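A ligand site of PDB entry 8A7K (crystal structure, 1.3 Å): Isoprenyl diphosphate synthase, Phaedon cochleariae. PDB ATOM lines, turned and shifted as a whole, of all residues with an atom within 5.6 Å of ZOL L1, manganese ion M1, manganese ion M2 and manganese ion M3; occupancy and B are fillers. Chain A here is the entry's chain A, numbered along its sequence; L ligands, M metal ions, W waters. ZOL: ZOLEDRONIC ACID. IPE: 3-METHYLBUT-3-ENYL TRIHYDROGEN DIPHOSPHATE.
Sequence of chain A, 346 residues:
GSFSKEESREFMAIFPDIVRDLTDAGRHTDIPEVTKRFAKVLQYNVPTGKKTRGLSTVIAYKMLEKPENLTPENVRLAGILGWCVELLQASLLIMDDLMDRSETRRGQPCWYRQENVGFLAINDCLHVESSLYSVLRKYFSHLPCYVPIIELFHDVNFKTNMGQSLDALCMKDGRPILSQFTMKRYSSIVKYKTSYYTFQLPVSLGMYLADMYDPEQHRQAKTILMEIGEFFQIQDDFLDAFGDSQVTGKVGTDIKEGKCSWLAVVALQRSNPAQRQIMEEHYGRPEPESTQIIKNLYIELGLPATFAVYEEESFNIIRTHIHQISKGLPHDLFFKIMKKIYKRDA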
ATOM      1  N   LEU A  92      -5.399 -24.022  -0.608  1.00  0.00           N
ATOM      2  CA  LEU A  92      -6.172 -22.763  -0.440  1.00  0.00           C
ATOM      3  C   LEU A  92      -6.919 -22.769   0.919  1.00  0.00           C
ATOM      4  O   LEU A  92      -7.032 -21.660   1.549  1.00  0.00           O
ATOM      5  CB  LEU A  92      -7.160 -22.627  -1.594  1.00  0.00           C
ATOM      6  CG  LEU A  92      -6.485 -22.356  -2.946  1.00  0.00           C
ATOM      7  CD1 LEU A  92      -7.507 -22.553  -4.060  1.00  0.00           C
ATOM      8  CD2 LEU A  92      -5.941 -20.901  -2.985  1.00  0.00           C
ATOM      9  N   LEU A  93      -7.453 -23.928   1.364  1.00  0.00           N
ATOM     10  CA  LEU A  93      -8.231 -23.988   2.616  1.00  0.00           C
ATOM     11  C   LEU A  93      -7.320 -23.751   3.826  1.00  0.00           C
ATOM     12  O   LEU A  93      -7.754 -23.131   4.770  1.00  0.00           O
ATOM     13  CB  LEU A  93      -9.076 -25.241   2.723  1.00  0.00           C
ATOM     14  CG  LEU A  93     -10.092 -25.441   1.578  1.00  0.00           C
ATOM     15  CD1 LEU A  93     -10.940 -26.671   1.889  1.00  0.00           C
ATOM     16  CD2 LEU A  93     -10.944 -24.198   1.321  1.00  0.00           C
ATOM     17  N   ASP A  96      -6.812 -20.112   3.837  1.00  0.00           N
ATOM     18  CA  ASP A  96      -8.087 -19.406   4.041  1.00  0.00           C
ATOM     19  C   ASP A  96      -8.520 -19.445   5.517  1.00  0.00           C
ATOM     20  O   ASP A  96      -8.995 -18.437   6.046  1.00  0.00           O
ATOM     21  CB  ASP A  96      -9.101 -20.011   3.098  1.00  0.00           C
ATOM     22  CG  ASP A  96     -10.425 -19.341   3.274  1.00  0.00           C
ATOM     23  OD1 ASP A  96     -10.567 -18.208   2.649  1.00  0.00           O
ATOM     24  OD2 ASP A  96     -11.281 -19.765   3.997  1.00  0.00           O
ATOM     25  N   ASP A  97      -8.322 -20.590   6.133  1.00  0.00           N
ATOM     26  CA  ASP A  97      -8.710 -20.738   7.539  1.00  0.00           C
ATOM     27  C   ASP A  97      -7.863 -19.847   8.465  1.00  0.00           C
ATOM     28  O   ASP A  97      -8.407 -19.280   9.410  1.00  0.00           O
ATOM     29  CB  ASP A  97      -8.666 -22.221   7.927  1.00  0.00           C
ATOM     30  CG  ASP A  97      -9.856 -22.975   7.357  1.00  0.00           C
ATOM     31  OD1 ASP A  97     -10.870 -22.359   7.055  1.00  0.00           O
ATOM     32  OD2 ASP A  97      -9.694 -24.263   7.273  1.00  0.00           O
ATOM     33  N   ASP A 100      -9.233 -16.259   7.806  1.00  0.00           N
ATOM     34  CA  ASP A 100     -10.631 -16.092   8.262  1.00  0.00           C
ATOM     35  C   ASP A 100     -10.737 -16.371   9.745  1.00  0.00           C
ATOM     36  O   ASP A 100     -11.851 -16.241  10.267  1.00  0.00           O
ATOM     37  CB  ASP A 100     -11.529 -16.920   7.380  1.00  0.00           C
ATOM     38  CG  ASP A 100     -11.573 -16.432   5.979  1.00  0.00           C
ATOM     39  OD1 ASP A 100     -11.139 -15.322   5.723  1.00  0.00           O
ATOM     40  OD2 ASP A 100     -12.166 -17.284   5.063  1.00  0.00           O
ATOM     41  N   SER A 102     -10.774 -19.095  11.351  1.00  0.00           N
ATOM     42  CA  SER A 102     -11.807 -20.153  11.483  1.00  0.00           C
ATOM     43  C   SER A 102     -11.449 -21.159  12.563  1.00  0.00           C
ATOM     44  O   SER A 102     -10.306 -21.264  12.973  1.00  0.00           O
ATOM     45  CB  SER A 102     -12.029 -20.775  10.095  1.00  0.00           C
ATOM     46  OG  SER A 102     -12.669 -19.830   9.214  1.00  0.00           O
ATOM     47  N   ARG A 105     -12.660 -27.145  10.141  1.00  0.00           N
ATOM     48  CA  ARG A 105     -12.653 -27.407   8.698  1.00  0.00           C
ATOM     49  C   ARG A 105     -12.853 -28.897   8.504  1.00  0.00           C
ATOM     50  O   ARG A 105     -12.132 -29.662   9.121  1.00  0.00           O
ATOM     51  CB  ARG A 105     -11.321 -26.988   8.108  1.00  0.00           C
ATOM     52  CG  ARG A 105     -11.148 -27.404   6.659  1.00  0.00           C
ATOM     53  CD  ARG A 105     -12.049 -26.741   5.628  1.00  0.00           C
ATOM     54  NE  ARG A 105     -11.782 -25.326   5.518  1.00  0.00           N
ATOM     55  CZ  ARG A 105     -12.487 -24.504   4.754  1.00  0.00           C
ATOM     56  NH1 ARG A 105     -13.528 -24.923   4.055  1.00  0.00           N
ATOM     57  NH2 ARG A 105     -12.180 -23.209   4.725  1.00  0.00           N
ATOM     58  N   THR A 160      -6.995 -16.871  -8.592  1.00  0.00           N
ATOM     59  CA  THR A 160      -7.559 -17.220  -7.249  1.00  0.00           C
ATOM     60  C   THR A 160      -6.960 -16.245  -6.217  1.00  0.00           C
ATOM     61  O   THR A 160      -7.695 -15.779  -5.368  1.00  0.00           O
ATOM     62  CB  THR A 160      -7.306 -18.689  -6.916  1.00  0.00           C
ATOM     63  OG1 THR A 160      -7.864 -19.517  -7.947  1.00  0.00           O
ATOM     64  CG2 THR A 160      -7.971 -19.029  -5.615  1.00  0.00           C
ATOM     65  N   GLN A 164      -8.996 -13.810  -3.680  1.00  0.00           N
ATOM     66  CA  GLN A 164      -8.762 -13.874  -2.218  1.00  0.00           C
ATOM     67  C   GLN A 164      -8.451 -12.489  -1.696  1.00  0.00           C
ATOM     68  O   GLN A 164      -8.868 -12.123  -0.602  1.00  0.00           O
ATOM     69  CB  GLN A 164      -7.720 -14.916  -1.898  1.00  0.00           C
ATOM     70  CG  GLN A 164      -7.605 -15.237  -0.440  1.00  0.00           C
ATOM     71  CD  GLN A 164      -8.718 -16.155   0.059  1.00  0.00           C
ATOM     72  OE1 GLN A 164      -9.761 -16.447  -0.642  1.00  0.00           O
ATOM     73  NE2 GLN A 164      -8.449 -16.650   1.275  1.00  0.00           N
ATOM     74  N   ASP A 167     -11.708 -10.326  -1.795  1.00  0.00           N
ATOM     75  CA  ASP A 167     -12.502 -10.809  -0.662  1.00  0.00           C
ATOM     76  C   ASP A 167     -12.030 -10.164   0.645  1.00  0.00           C
ATOM     77  O   ASP A 167     -12.870  -9.818   1.518  1.00  0.00           O
ATOM     78  CB  ASP A 167     -12.405 -12.313  -0.618  1.00  0.00           C
ATOM     79  CG  ASP A 167     -13.144 -12.987   0.514  1.00  0.00           C
ATOM     80  OD1 ASP A 167     -12.597 -13.056   1.597  1.00  0.00           O
ATOM     81  OD2 ASP A 167     -14.316 -13.374   0.295  1.00  0.00           O
ATOM     82  N   LYS A 193     -12.245 -15.735  -6.751  1.00  0.00           N
ATOM     83  CA  LYS A 193     -11.844 -16.543  -5.559  1.00  0.00           C
ATOM     84  C   LYS A 193     -12.323 -17.975  -5.605  1.00  0.00           C
ATOM     85  O   LYS A 193     -11.797 -18.791  -4.847  1.00  0.00           O
ATOM     86  CB  LYS A 193     -12.237 -15.888  -4.236  1.00  0.00           C
ATOM     87  CG  LYS A 193     -13.689 -16.028  -3.833  1.00  0.00           C
ATOM     88  CD  LYS A 193     -13.922 -15.799  -2.391  1.00  0.00           C
ATOM     89  CE  LYS A 193     -15.383 -15.929  -2.023  1.00  0.00           C
ATOM     90  NZ  LYS A 193     -15.621 -15.721  -0.574  1.00  0.00           N
ATOM     91  N   THR A 194     -13.346 -18.257  -6.457  1.00  0.00           N
ATOM     92  CA  THR A 194     -13.935 -19.593  -6.436  1.00  0.00           C
ATOM     93  C   THR A 194     -14.140 -20.173  -7.859  1.00  0.00           C
ATOM     94  O   THR A 194     -13.800 -21.338  -8.044  1.00  0.00           O
ATOM     95  CB  THR A 194     -15.260 -19.523  -5.686  1.00  0.00           C
ATOM     96  OG1 THR A 194     -14.951 -19.390  -4.304  1.00  0.00           O
ATOM     97  CG2 THR A 194     -16.131 -20.766  -5.920  1.00  0.00           C
ATOM     98  N   TYR A 197     -11.075 -21.901 -10.080  1.00  0.00           N
ATOM     99  CA  TYR A 197     -10.417 -23.146  -9.626  1.00  0.00           C
ATOM    100  C   TYR A 197     -11.418 -24.228  -9.329  1.00  0.00           C
ATOM    101  O   TYR A 197     -11.042 -25.429  -9.408  1.00  0.00           O
ATOM    102  CB  TYR A 197      -9.506 -22.906  -8.406  1.00  0.00           C
ATOM    103  CG  TYR A 197     -10.168 -23.030  -7.041  1.00  0.00           C
ATOM    104  CD1 TYR A 197     -10.793 -22.010  -6.396  1.00  0.00           C
ATOM    105  CD2 TYR A 197     -10.069 -24.233  -6.371  1.00  0.00           C
ATOM    106  CE1 TYR A 197     -11.322 -22.158  -5.112  1.00  0.00           C
ATOM    107  CE2 TYR A 197     -10.583 -24.414  -5.097  1.00  0.00           C
ATOM    108  CZ  TYR A 197     -11.259 -23.383  -4.474  1.00  0.00           C
ATOM    109  OH  TYR A 197     -11.757 -23.495  -3.204  1.00  0.00           O
ATOM    110  N   GLN A 233     -20.944 -20.441  -4.810  1.00  0.00           N
ATOM    111  CA  GLN A 233     -20.486 -19.559  -3.731  1.00  0.00           C
ATOM    112  C   GLN A 233     -21.646 -18.925  -2.946  1.00  0.00           C
ATOM    113  O   GLN A 233     -21.511 -18.764  -1.726  1.00  0.00           O
ATOM    114  CB  GLN A 233     -19.500 -18.526  -4.233  1.00  0.00           C
ATOM    115  CG  GLN A 233     -18.820 -17.725  -3.091  1.00  0.00           C
ATOM    116  CD  GLN A 233     -17.930 -18.594  -2.223  1.00  0.00           C
ATOM    117  OE1 GLN A 233     -17.142 -19.375  -2.734  1.00  0.00           O
ATOM    118  NE2 GLN A 233     -18.088 -18.429  -0.921  1.00  0.00           N
ATOM    119  N   ASP A 236     -22.460 -21.465  -0.562  1.00  0.00           N
ATOM    120  CA  ASP A 236     -21.477 -21.460   0.544  1.00  0.00           C
ATOM    121  C   ASP A 236     -21.794 -20.366   1.577  1.00  0.00           C
ATOM    122  O   ASP A 236     -21.639 -20.540   2.773  1.00  0.00           O
ATOM    123  CB  ASP A 236     -20.071 -21.291  -0.005  1.00  0.00           C
ATOM    124  CG  ASP A 236     -19.051 -21.423   1.084  1.00  0.00           C
ATOM    125  OD1 ASP A 236     -18.900 -22.531   1.646  1.00  0.00           O
ATOM    126  OD2 ASP A 236     -18.354 -20.406   1.379  1.00  0.00           O
ATOM    127  N   ASP A 237     -22.105 -19.172   1.043  1.00  0.00           N
ATOM    128  CA  ASP A 237     -22.360 -18.041   1.946  1.00  0.00           C
ATOM    129  C   ASP A 237     -23.585 -18.344   2.809  1.00  0.00           C
ATOM    130  O   ASP A 237     -23.631 -17.940   3.973  1.00  0.00           O
ATOM    131  CB  ASP A 237     -22.521 -16.764   1.136  1.00  0.00           C
ATOM    132  CG  ASP A 237     -21.291 -16.342   0.380  1.00  0.00           C
ATOM    133  OD1 ASP A 237     -20.209 -16.912   0.558  1.00  0.00           O
ATOM    134  OD2 ASP A 237     -21.439 -15.338  -0.380  1.00  0.00           O
ATOM    135  N   ASP A 240     -22.584 -20.437   5.677  1.00  0.00           N
ATOM    136  CA  ASP A 240     -21.752 -19.786   6.716  1.00  0.00           C
ATOM    137  C   ASP A 240     -22.674 -19.413   7.910  1.00  0.00           C
ATOM    138  O   ASP A 240     -22.307 -19.617   9.056  1.00  0.00           O
ATOM    139  CB  ASP A 240     -21.066 -18.559   6.148  1.00  0.00           C
ATOM    140  CG  ASP A 240     -20.073 -17.991   7.168  1.00  0.00           C
ATOM    141  OD1 ASP A 240     -18.915 -18.460   7.162  1.00  0.00           O
ATOM    142  OD2 ASP A 240     -20.488 -17.075   7.895  1.00  0.00           O
ATOM    143  N   LYS A 250     -17.782 -26.991   9.311  1.00  0.00           N
ATOM    144  CA  LYS A 250     -17.086 -25.715   9.508  1.00  0.00           C
ATOM    145  C   LYS A 250     -18.030 -24.745  10.214  1.00  0.00           C
ATOM    146  O   LYS A 250     -19.232 -24.696   9.963  1.00  0.00           O
ATOM    147  CB  LYS A 250     -16.520 -25.143   8.205  1.00  0.00           C
ATOM    148  CG  LYS A 250     -17.572 -24.819   7.137  1.00  0.00           C
ATOM    149  CD  LYS A 250     -16.918 -24.555   5.788  1.00  0.00           C
ATOM    150  CE  LYS A 250     -17.896 -23.993   4.785  1.00  0.00           C
ATOM    151  NZ  LYS A 250     -17.284 -23.836   3.463  1.00  0.00           N
ATOM    152  N   THR A 253     -17.817 -17.642   9.869  1.00  0.00           N
ATOM    153  CA  THR A 253     -17.045 -16.441  10.311  1.00  0.00           C
ATOM    154  C   THR A 253     -17.348 -15.205   9.456  1.00  0.00           C
ATOM    155  O   THR A 253     -16.773 -14.185   9.723  1.00  0.00           O
ATOM    156  CB  THR A 253     -15.542 -16.681  10.257  1.00  0.00           C
ATOM    157  OG1 THR A 253     -15.164 -17.009   8.908  1.00  0.00           O
ATOM    158  CG2 THR A 253     -15.041 -17.706  11.223  1.00  0.00           C
ATOM    159  N   ASP A 254     -18.230 -15.246   8.464  1.00  0.00           N
ATOM    160  CA  ASP A 254     -18.346 -14.104   7.550  1.00  0.00           C
ATOM    161  C   ASP A 254     -18.794 -12.871   8.297  1.00  0.00           C
ATOM    162  O   ASP A 254     -18.388 -11.748   7.933  1.00  0.00           O
ATOM    163  CB  ASP A 254     -19.289 -14.441   6.407  1.00  0.00           C
ATOM    164  CG  ASP A 254     -18.740 -15.461   5.426  1.00  0.00           C
ATOM    165  OD1 ASP A 254     -17.516 -15.668   5.381  1.00  0.00           O
ATOM    166  OD2 ASP A 254     -19.540 -15.997   4.589  1.00  0.00           O
ATOM    167  N   LYS A 259     -17.417  -9.758   5.964  1.00  0.00           N
ATOM    168  CA  LYS A 259     -17.291 -10.081   4.537  1.00  0.00           C
ATOM    169  C   LYS A 259     -18.428  -9.578   3.664  1.00  0.00           C
ATOM    170  O   LYS A 259     -19.591  -9.526   4.120  1.00  0.00           O
ATOM    171  CB  LYS A 259     -17.274 -11.591   4.406  1.00  0.00           C
ATOM    172  CG  LYS A 259     -16.002 -12.228   4.982  1.00  0.00           C
ATOM    173  CD  LYS A 259     -14.781 -11.995   4.111  1.00  0.00           C
ATOM    174  CE  LYS A 259     -13.436 -12.035   4.776  1.00  0.00           C
ATOM    175  NZ  LYS A 259     -13.240 -13.358   5.400  1.00  0.00           N
HETATM  176  O17 ZOL L   1     -14.403 -17.797   0.610  1.00  0.00           O
HETATM  177  P14 ZOL L   1     -14.681 -18.528   1.925  1.00  0.00           P
HETATM  178  O16 ZOL L   1     -13.538 -18.071   2.978  1.00  0.00           O
HETATM  179  O15 ZOL L   1     -16.156 -18.349   2.411  1.00  0.00           O
HETATM  180  C8  ZOL L   1     -14.568 -20.331   1.659  1.00  0.00           C
HETATM  181  P9  ZOL L   1     -14.919 -21.293   3.193  1.00  0.00           P
HETATM  182  O10 ZOL L   1     -16.360 -21.013   3.506  1.00  0.00           O
HETATM  183  O11 ZOL L   1     -14.034 -20.840   4.319  1.00  0.00           O
HETATM  184  O12 ZOL L   1     -14.715 -22.746   2.920  1.00  0.00           O
HETATM  185  O13 ZOL L   1     -15.514 -20.723   0.661  1.00  0.00           O
HETATM  186  C7  ZOL L   1     -13.177 -20.684   1.140  1.00  0.00           C
HETATM  187  N15 ZOL L   1     -12.814 -20.155  -0.173  1.00  0.00           N
HETATM  188  C16 ZOL L   1     -13.492 -20.197  -1.309  1.00  0.00           C
HETATM  189  N17 ZOL L   1     -12.856 -19.559  -2.299  1.00  0.00           N
HETATM  190  C18 ZOL L   1     -11.665 -19.155  -1.726  1.00  0.00           C
HETATM  191  C19 ZOL L   1     -11.594 -19.490  -0.452  1.00  0.00           C
HETATM  192  C1  IPE L   2     -15.113 -24.983  -0.036  1.00  0.00           C
HETATM  193  O1  IPE L   2     -15.357 -25.952  -1.050  1.00  0.00           O
HETATM  194  C2  IPE L   2     -14.633 -23.678  -0.634  1.00  0.00           C
HETATM  195  C3  IPE L   2     -15.532 -23.025  -1.650  1.00  0.00           C
HETATM  196  C4  IPE L   2     -15.096 -22.677  -2.852  1.00  0.00           C
HETATM  197  C5  IPE L   2     -16.976 -22.877  -1.282  1.00  0.00           C
HETATM  198  PA  IPE L   2     -16.158 -27.269  -0.743  1.00  0.00           P
HETATM  199  O1A IPE L   2     -17.438 -26.958  -0.066  1.00  0.00           O
HETATM  200  O2A IPE L   2     -16.263 -27.978  -2.041  1.00  0.00           O
HETATM  201  O3A IPE L   2     -15.227 -28.031   0.320  1.00  0.00           O
HETATM  202  PB  IPE L   2     -14.561 -29.518   0.413  1.00  0.00           P
HETATM  203  O1B IPE L   2     -14.292 -29.662   1.890  1.00  0.00           O
HETATM  204  O2B IPE L   2     -15.586 -30.443  -0.062  1.00  0.00           O
HETATM  205  O3B IPE L   2     -13.299 -29.518  -0.381  1.00  0.00           O
HETATM  206 MN    MN M   1     -13.110 -19.177   4.831  1.00  0.00          MN
HETATM  207 MN    MN M   2     -12.027 -16.647   2.928  1.00  0.00          MN
HETATM  208 MN    MN M   3     -17.662 -19.460   3.168  1.00  0.00          MN
HETATM  209  O   HOH W   1     -10.545 -15.412   3.165  1.00  0.00           O
HETATM  210  O   HOH W   2     -19.146 -20.582   4.172  1.00  0.00           O
HETATM  211  O   HOH W   3     -12.113 -16.405   0.872  1.00  0.00           O
HETATM  212  O   HOH W   4     -17.291 -18.485   5.075  1.00  0.00           O
HETATM  213  O   HOH W   5     -15.230 -21.600   6.701  1.00  0.00           O
HETATM  214  O   HOH W   6     -13.501 -15.138   3.140  1.00  0.00           O
HETATM  215  O   HOH W   7     -14.644 -18.316   5.911  1.00  0.00           O
HETATM  216  O   HOH W   8     -19.014 -17.912   2.803  1.00  0.00           O
HETATM  217  O   HOH W   9     -12.271 -20.044   6.557  1.00  0.00           O
HETATM  218  O   HOH W  10     -16.240 -15.624   2.965  1.00  0.00           O
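Manganese ion M2 is bound by water W1 (1.9 Å). Water W3 is bound to manganese ion M2 (2.1 Å). Manganese ion M2 is bound by O16 of ZOL L1, 2.1 Å away. Water W6 is bound to manganese ion M2. Manganese ion M2 is bound by OD1 of Asp 96 (2.2 Å). Manganese ion M2 is bound by OD2 of Asp 100.
Water W9 bridges OG of Ser 102 and OD1 of Asp 97. Water W3 lies within hydrogen-bond range of an oxygen (O17) of ZOL L1, the side-chain amide oxygen (OE1) of Gln 164 and the side-chain carboxylate (OD1) of Asp 167. Water W1 lies within hydrogen-bond range of OD1 of Asp 100 (2.6 Å), NE2 of Gln 164 (3.1 Å) and OD1 of Asp 167 (3.5 Å). Water W6 bridges OD1 of Asp 167 (2.7 Å) and NZ of Lys 259 (2.9 Å). Water W4 lies within hydrogen-bond range of the side-chain carboxylate of Asp 240 and the side-chain carboxylate of Asp 254. Water W8 bridges OD2 of Asp 254 (2.7 Å) and OD1 of Asp 237 (2.7 Å).
Manganese ion M1 is bound by an oxygen (O11) of ZOL L1 (2.0 Å), water W7 (2.1 Å), the side-chain carboxylate of Asp 96 (2.1 Å), water W9 (2.1 Å), the side-chain carboxylate of Asp 100 (2.1 Å) and an oxygen (O16) of ZOL L1 (2.2 Å).
Residues that only touch manganese ion M2: Asp 167 and Gln 164. Of the 21 residues printed, 4 come within 4 Å of manganese ion M2.
OD1 of Asp 236 lies within salt-bridge range of NZ of Lys 250 (2.8 Å). The side-chain amide nitrogen of Gln 233 sits at hydrogen-bond distance from the side-chain carboxylate of Asp 237, at 3.0 Å. The side-chain hydroxyl (OG1) of Thr 194 sits at hydrogen-bond distance from the side-chain amide oxygen (OE1) of Gln 233, 2.7 Å away. OD1 of Asp 97 lies within salt-bridge range of NH2 of Arg 105 (2.8 Å). NZ of Lys 193 is in salt-bridge range of OD2 of Asp 167 (2.8 Å). The side-chain carboxylate of Asp 96 lies close to the side-chain amide nitrogen of Gln 164, at 3.0 Å. OD2 of Asp 236 sits close to NE2 of Gln 233 (3.0 Å). The side-chain carboxylate (OD2) of Asp 96 lies close to the guanidinium group (NH2) of Arg 105 (3.6 Å).
The side-chain amino group (NZ) of Lys 250 lies within salt-bridge range of an oxygen (O12) of ZOL L1 (2.8 Å). OG1 of Thr 194 lies within hydrogen-bond range of N17 of ZOL L1, at 2.9 Å. O12 of ZOL L1 lies within salt-bridge range of NH1 of Arg 105. O17 of ZOL L1 is in salt-bridge range of NZ of Lys 193 (2.7 Å).
Manganese ion M3 is bound by O15 of ZOL L1 (2.0 Å). O10 of ZOL L1 binds manganese ion M3 (2.1 Å). Manganese ion M3 is bound by water W8, 2.1 Å away. Manganese ion M3 is bound by water W2, at 2.1 Å. OD2 of Asp 236 is bound to manganese ion M3. Water W4 is bound to manganese ion M3. Manganese ion M3 has six donor atoms within binding distance.
Merely in contact with ZOL L1: Gln 164 (3.5 Å) and Gln 233 (3.8 Å). Within 4 Å of ZOL L1: Asp 96, Asp 100, Arg 105, Gln 164, Lys 193, Thr 194, Gln 233, Asp 236 and Lys 250. Along chain A the residues within 4 Å of ZOL L1 span positions 96 to 250.
Of the 21 residues printed, 1 comes within 4 Å of manganese ion M3. The nearest printed residue that does not touch manganese ion M3 is Asp 254 (4.2 Å).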
